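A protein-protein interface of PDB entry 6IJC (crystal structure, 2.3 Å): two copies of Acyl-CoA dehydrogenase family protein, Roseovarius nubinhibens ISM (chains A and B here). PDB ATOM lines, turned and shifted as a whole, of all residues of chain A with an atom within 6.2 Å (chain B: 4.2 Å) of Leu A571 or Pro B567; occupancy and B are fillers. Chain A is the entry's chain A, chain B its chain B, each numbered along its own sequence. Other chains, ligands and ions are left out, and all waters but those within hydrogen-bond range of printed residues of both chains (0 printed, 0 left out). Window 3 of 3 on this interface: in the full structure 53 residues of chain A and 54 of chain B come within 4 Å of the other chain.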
ATOM      1  N   ASP A 516      25.563 -22.366  35.707  1.00  0.00           N
ATOM      2  CA  ASP A 516      24.348 -21.615  35.420  1.00  0.00           C
ATOM      3  C   ASP A 516      23.939 -20.727  36.583  1.00  0.00           C
ATOM      4  O   ASP A 516      23.421 -19.622  36.367  1.00  0.00           O
ATOM      5  CB  ASP A 516      23.228 -22.582  35.074  1.00  0.00           C
ATOM      6  CG  ASP A 516      23.350 -23.088  33.675  1.00  0.00           C
ATOM      7  OD1 ASP A 516      23.222 -22.267  32.725  1.00  0.00           O
ATOM      8  OD2 ASP A 516      23.601 -24.298  33.520  1.00  0.00           O
ATOM      9  N   PRO A 567      16.371 -11.280  31.037  1.00  0.00           N
ATOM     10  CA  PRO A 567      15.580 -12.517  30.876  1.00  0.00           C
ATOM     11  C   PRO A 567      16.408 -13.792  30.804  1.00  0.00           C
ATOM     12  O   PRO A 567      15.845 -14.881  30.896  1.00  0.00           O
ATOM     13  CB  PRO A 567      14.831 -12.296  29.549  1.00  0.00           C
ATOM     14  CG  PRO A 567      14.729 -10.827  29.409  1.00  0.00           C
ATOM     15  CD  PRO A 567      16.020 -10.286  29.999  1.00  0.00           C
ATOM     16  N   ALA A 568      17.726 -13.683  30.605  1.00  0.00           N
ATOM     17  CA  ALA A 568      18.570 -14.867  30.578  1.00  0.00           C
ATOM     18  C   ALA A 568      18.508 -15.672  31.879  1.00  0.00           C
ATOM     19  O   ALA A 568      18.841 -16.862  31.857  1.00  0.00           O
ATOM     20  CB  ALA A 568      20.020 -14.471  30.263  1.00  0.00           C
ATOM     21  N   THR A 569      18.076 -15.062  32.998  1.00  0.00           N
ATOM     22  CA  THR A 569      17.899 -15.807  34.249  1.00  0.00           C
ATOM     23  C   THR A 569      16.927 -16.964  34.081  1.00  0.00           C
ATOM     24  O   THR A 569      17.014 -17.958  34.810  1.00  0.00           O
ATOM     25  CB  THR A 569      17.374 -14.909  35.394  1.00  0.00           C
ATOM     26  OG1 THR A 569      16.082 -14.400  35.055  1.00  0.00           O
ATOM     27  CG2 THR A 569      18.309 -13.760  35.698  1.00  0.00           C
ATOM     28  N   LYS A 570      15.971 -16.835  33.162  1.00  0.00           N
ATOM     29  CA  LYS A 570      15.013 -17.917  32.956  1.00  0.00           C
ATOM     30  C   LYS A 570      15.682 -19.129  32.320  1.00  0.00           C
ATOM     31  O   LYS A 570      15.401 -20.273  32.699  1.00  0.00           O
ATOM     32  CB  LYS A 570      13.841 -17.423  32.111  1.00  0.00           C
ATOM     33  CG  LYS A 570      12.961 -16.418  32.846  1.00  0.00           C
ATOM     34  CD  LYS A 570      11.859 -15.870  31.932  1.00  0.00           C
ATOM     35  CE  LYS A 570      12.053 -14.387  31.639  1.00  0.00           C
ATOM     36  NZ  LYS A 570      11.046 -13.531  32.355  1.00  0.00           N
ATOM     37  N   LEU A 571      16.597 -18.904  31.377  1.00  0.00           N
ATOM     38  CA  LEU A 571      17.328 -20.030  30.808  1.00  0.00           C
ATOM     39  C   LEU A 571      18.236 -20.682  31.854  1.00  0.00           C
ATOM     40  O   LEU A 571      18.360 -21.914  31.907  1.00  0.00           O
ATOM     41  CB  LEU A 571      18.131 -19.568  29.592  1.00  0.00           C
ATOM     42  CG  LEU A 571      18.987 -20.649  28.921  1.00  0.00           C
ATOM     43  CD1 LEU A 571      18.162 -21.904  28.642  1.00  0.00           C
ATOM     44  CD2 LEU A 571      19.600 -20.113  27.647  1.00  0.00           C
ATOM     45  N   HIS A 572      18.860 -19.872  32.711  1.00  0.00           N
ATOM     46  CA  HIS A 572      19.751 -20.444  33.710  1.00  0.00           C
ATOM     47  C   HIS A 572      18.972 -21.243  34.746  1.00  0.00           C
ATOM     48  O   HIS A 572      19.413 -22.321  35.156  1.00  0.00           O
ATOM     49  CB  HIS A 572      20.600 -19.331  34.322  1.00  0.00           C
ATOM     50  CG  HIS A 572      21.548 -18.725  33.336  1.00  0.00           C
ATOM     51  ND1 HIS A 572      22.501 -19.477  32.671  1.00  0.00           N
ATOM     52  CD2 HIS A 572      21.652 -17.467  32.845  1.00  0.00           C
ATOM     53  CE1 HIS A 572      23.172 -18.700  31.840  1.00  0.00           C
ATOM     54  NE2 HIS A 572      22.674 -17.478  31.925  1.00  0.00           N
ATOM     55  N   LEU A 573      17.788 -20.760  35.140  1.00  0.00           N
ATOM     56  CA  LEU A 573      16.950 -21.522  36.062  1.00  0.00           C
ATOM     57  C   LEU A 573      16.569 -22.878  35.468  1.00  0.00           C
ATOM     58  O   LEU A 573      16.703 -23.913  36.126  1.00  0.00           O
ATOM     59  CB  LEU A 573      15.698 -20.714  36.440  1.00  0.00           C
ATOM     60  CG  LEU A 573      14.697 -21.388  37.394  1.00  0.00           C
ATOM     61  CD1 LEU A 573      15.406 -21.976  38.619  1.00  0.00           C
ATOM     62  CD2 LEU A 573      13.587 -20.430  37.826  1.00  0.00           C
ATOM     63  N   ALA A 574      16.109 -22.892  34.214  1.00  0.00           N
ATOM     64  CA  ALA A 574      15.725 -24.151  33.570  1.00  0.00           C
ATOM     65  C   ALA A 574      16.868 -25.156  33.577  1.00  0.00           C
ATOM     66  O   ALA A 574      16.650 -26.348  33.815  1.00  0.00           O
ATOM     67  CB  ALA A 574      15.260 -23.894  32.138  1.00  0.00           C
ATOM     68  N   ARG A 575      18.092 -24.697  33.311  1.00  0.00           N
ATOM     69  CA  ARG A 575      19.241 -25.589  33.257  1.00  0.00           C
ATOM     70  C   ARG A 575      19.682 -26.047  34.642  1.00  0.00           C
ATOM     71  O   ARG A 575      20.378 -27.064  34.754  1.00  0.00           O
ATOM     72  CB  ARG A 575      20.396 -24.900  32.527  1.00  0.00           C
ATOM     73  CG  ARG A 575      20.205 -24.816  31.026  1.00  0.00           C
ATOM     74  CD  ARG A 575      21.224 -23.883  30.345  1.00  0.00           C
ATOM     75  NE  ARG A 575      22.623 -24.242  30.613  1.00  0.00           N
ATOM     76  CZ  ARG A 575      23.316 -25.167  29.953  1.00  0.00           C
ATOM     77  NH1 ARG A 575      22.751 -25.876  28.977  1.00  0.00           N
ATOM     78  NH2 ARG A 575      24.582 -25.399  30.282  1.00  0.00           N
ATOM     79  N   ILE A 576      19.284 -25.328  35.687  1.00  0.00           N
ATOM     80  CA  ILE A 576      19.527 -25.765  37.057  1.00  0.00           C
ATOM     81  C   ILE A 576      18.480 -26.785  37.502  1.00  0.00           C
ATOM     82  O   ILE A 576      18.813 -27.813  38.107  1.00  0.00           O
ATOM     83  CB  ILE A 576      19.548 -24.547  37.999  1.00  0.00           C
ATOM     84  CG1 ILE A 576      20.789 -23.690  37.741  1.00  0.00           C
ATOM     85  CG2 ILE A 576      19.464 -24.997  39.469  1.00  0.00           C
ATOM     86  CD1 ILE A 576      20.766 -22.372  38.501  1.00  0.00           C
ATOM     87  N   MET B 562      16.846 -31.278  25.059  1.00  0.00           N
ATOM     88  CA  MET B 562      15.491 -30.769  25.261  1.00  0.00           C
ATOM     89  C   MET B 562      15.373 -29.954  26.543  1.00  0.00           C
ATOM     90  O   MET B 562      14.629 -28.971  26.589  1.00  0.00           O
ATOM     91  CB  MET B 562      14.478 -31.917  25.301  1.00  0.00           C
ATOM     92  CG  MET B 562      14.396 -32.782  24.047  1.00  0.00           C
ATOM     93  SD  MET B 562      14.168 -31.863  22.508  1.00  0.00           S
ATOM     94  CE  MET B 562      13.617 -33.189  21.426  1.00  0.00           C
ATOM     95  N   THR B 563      16.066 -30.365  27.603  1.00  0.00           N
ATOM     96  CA  THR B 563      15.891 -29.741  28.904  1.00  0.00           C
ATOM     97  C   THR B 563      16.930 -28.671  29.202  1.00  0.00           C
ATOM     98  O   THR B 563      16.654 -27.787  30.018  1.00  0.00           O
ATOM     99  CB  THR B 563      15.918 -30.809  30.018  1.00  0.00           C
ATOM    100  OG1 THR B 563      17.107 -31.589  29.895  1.00  0.00           O
ATOM    101  CG2 THR B 563      14.708 -31.756  29.908  1.00  0.00           C
ATOM    102  N   ARG B 564      18.099 -28.716  28.550  1.00  0.00           N
ATOM    103  CA  ARG B 564      19.205 -27.811  28.858  1.00  0.00           C
ATOM    104  C   ARG B 564      19.526 -26.802  27.765  1.00  0.00           C
ATOM    105  O   ARG B 564      20.074 -25.747  28.072  1.00  0.00           O
ATOM    106  CB  ARG B 564      20.494 -28.596  29.156  1.00  0.00           C
ATOM    107  CG  ARG B 564      20.666 -29.026  30.612  1.00  0.00           C
ATOM    108  CD  ARG B 564      19.740 -30.188  30.942  1.00  0.00           C
ATOM    109  NE  ARG B 564      20.296 -31.080  31.966  1.00  0.00           N
ATOM    110  CZ  ARG B 564      19.716 -32.205  32.379  1.00  0.00           C
ATOM    111  NH1 ARG B 564      18.550 -32.586  31.868  1.00  0.00           N
ATOM    112  NH2 ARG B 564      20.303 -32.955  33.298  1.00  0.00           N
ATOM    113  N   ARG B 565      19.261 -27.104  26.500  1.00  0.00           N
ATOM    114  CA  ARG B 565      19.618 -26.183  25.425  1.00  0.00           C
ATOM    115  C   ARG B 565      18.396 -25.578  24.754  1.00  0.00           C
ATOM    116  O   ARG B 565      18.335 -24.355  24.581  1.00  0.00           O
ATOM    117  CB  ARG B 565      20.519 -26.887  24.392  1.00  0.00           C
ATOM    118  CG  ARG B 565      21.829 -27.391  25.031  1.00  0.00           C
ATOM    119  CD  ARG B 565      22.988 -27.515  24.040  1.00  0.00           C
ATOM    120  NE  ARG B 565      23.318 -26.262  23.350  1.00  0.00           N
ATOM    121  CZ  ARG B 565      24.074 -25.295  23.869  1.00  0.00           C
ATOM    122  NH1 ARG B 565      24.571 -25.424  25.094  1.00  0.00           N
ATOM    123  NH2 ARG B 565      24.333 -24.199  23.167  1.00  0.00           N
ATOM    124  N   LEU B 566      17.414 -26.416  24.407  1.00  0.00           N
ATOM    125  CA  LEU B 566      16.161 -25.954  23.816  1.00  0.00           C
ATOM    126  C   LEU B 566      15.461 -24.847  24.601  1.00  0.00           C
ATOM    127  O   LEU B 566      14.830 -23.987  23.954  1.00  0.00           O
ATOM    128  CB  LEU B 566      15.218 -27.153  23.630  1.00  0.00           C
ATOM    129  CG  LEU B 566      14.009 -26.991  22.692  1.00  0.00           C
ATOM    130  CD1 LEU B 566      14.422 -26.580  21.264  1.00  0.00           C
ATOM    131  CD2 LEU B 566      13.196 -28.288  22.657  1.00  0.00           C
ATOM    132  N   PRO B 567      15.502 -24.787  25.941  1.00  0.00           N
ATOM    133  CA  PRO B 567      14.817 -23.676  26.628  1.00  0.00           C
ATOM    134  C   PRO B 567      15.357 -22.305  26.264  1.00  0.00           C
ATOM    135  O   PRO B 567      14.703 -21.316  26.601  1.00  0.00           O
ATOM    136  CB  PRO B 567      15.030 -23.976  28.121  1.00  0.00           C
ATOM    137  CG  PRO B 567      15.241 -25.453  28.175  1.00  0.00           C
ATOM    138  CD  PRO B 567      15.931 -25.831  26.903  1.00  0.00           C
ATOM    139  N   ALA B 568      16.512 -22.212  25.589  1.00  0.00           N
ATOM    140  CA  ALA B 568      16.990 -20.924  25.087  1.00  0.00           C
ATOM    141  C   ALA B 568      15.962 -20.203  24.210  1.00  0.00           C
ATOM    142  O   ALA B 568      15.999 -18.973  24.104  1.00  0.00           O
ATOM    143  CB  ALA B 568      18.287 -21.122  24.299  1.00  0.00           C
ATOM    144  N   THR B 569      15.044 -20.939  23.569  1.00  0.00           N
ATOM    145  CA  THR B 569      14.041 -20.294  22.729  1.00  0.00           C
ATOM    146  C   THR B 569      13.237 -19.252  23.510  1.00  0.00           C
ATOM    147  O   THR B 569      12.783 -18.260  22.929  1.00  0.00           O
ATOM    148  CB  THR B 569      13.096 -21.339  22.096  1.00  0.00           C
ATOM    149  OG1 THR B 569      12.338 -22.021  23.115  1.00  0.00           O
ATOM    150  CG2 THR B 569      13.868 -22.372  21.275  1.00  0.00           C
ATOM    151  N   LYS B 570      13.045 -19.458  24.819  1.00  0.00           N
ATOM    152  CA  LYS B 570      12.344 -18.463  25.634  1.00  0.00           C
ATOM    153  C   LYS B 570      13.137 -17.165  25.729  1.00  0.00           C
ATOM    154  O   LYS B 570      12.558 -16.067  25.692  1.00  0.00           O
ATOM    155  CB  LYS B 570      12.065 -19.024  27.027  1.00  0.00           C
ATOM    156  CG  LYS B 570      10.867 -19.948  27.064  1.00  0.00           C
ATOM    157  CD  LYS B 570      11.070 -21.091  28.045  1.00  0.00           C
ATOM    158  CE  LYS B 570      10.078 -22.225  27.773  1.00  0.00           C
ATOM    159  NZ  LYS B 570      10.025 -22.581  26.297  1.00  0.00           N
ATOM    160  N   LEU B 571      14.463 -17.266  25.825  1.00  0.00           N
ATOM    161  CA  LEU B 571      15.283 -16.062  25.890  1.00  0.00           C
ATOM    162  C   LEU B 571      15.256 -15.305  24.565  1.00  0.00           C
ATOM    163  O   LEU B 571      15.145 -14.072  24.541  1.00  0.00           O
ATOM    164  CB  LEU B 571      16.715 -16.432  26.264  1.00  0.00           C
ATOM    165  CG  LEU B 571      17.740 -15.294  26.201  1.00  0.00           C
ATOM    166  CD1 LEU B 571      17.296 -14.129  27.078  1.00  0.00           C
ATOM    167  CD2 LEU B 571      19.137 -15.790  26.622  1.00  0.00           C
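Pro A567 touches Leu B571, and with the chains exchanged Leu A571 touches Pro B567.
Ala A568 touches Leu B571, and with the chains exchanged Leu A571 touches Ala B568.
Of the 5 pairs that touch across the chains among the printed residues, 4 have their exchanged pair printed and touching as well.
Of chain B, only Pro B567 and Ala B568 come within 4 Å of Leu A571.
Pro B567 touches just one residue of chain A: Leu A571.
Of the printed residues of chain B, Pro A567 touches Leu B571.
Of the printed residues of chain A, Ala B568 touches Leu A571 (3.5 Å).
Printed residues of chain B within 4 Å of Arg A575: Arg B564 (2.8 Å).
Printed residues of chain B within 4 Å of Ala A568: Leu B571.
Thr B563 touches none of the printed residues of chain A.
Arg B565 touches none of the printed residues of chain A.
The nearest printed residue of chain B that does not touch Leu A571 is Arg B564 (4.3 Å).
Among the printed residues, pairs that only touch across the chains: Leu A571 with Ala B568 (3.5 Å), Ala A568 with Leu B571 (3.6 Å), Leu A571 with Pro B567 (3.7 Å) and Pro A567 with Leu B571 (3.8 Å).
The backbone carbonyl oxygen (O) of Arg B564 sits at hydrogen-bond distance from the guanidinium group (NH1) of Arg A575 (2.8 Å).
Printed residues of chain A that touch a printed residue of chain B: Pro A567, Ala A568, Leu A571 and Arg A575.
Of the 10 printed residues of chain B, 4 touch a printed residue of chain A.
Hydrophobic or aromatic side chains of chain B within 4 Å of the printed part of chain A: Pro B567, Ala B568 and Leu B571.
Among the printed residues, 5 pairs touch across the chains.
The guanidinium group of Arg B564 lies within hydrogen-bond range of the side-chain hydroxyl of Thr B563, at 2.6 Å.
NE of Arg A575 is in salt-bridge range of OD1 of Asp A516, 3.0 Å away.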
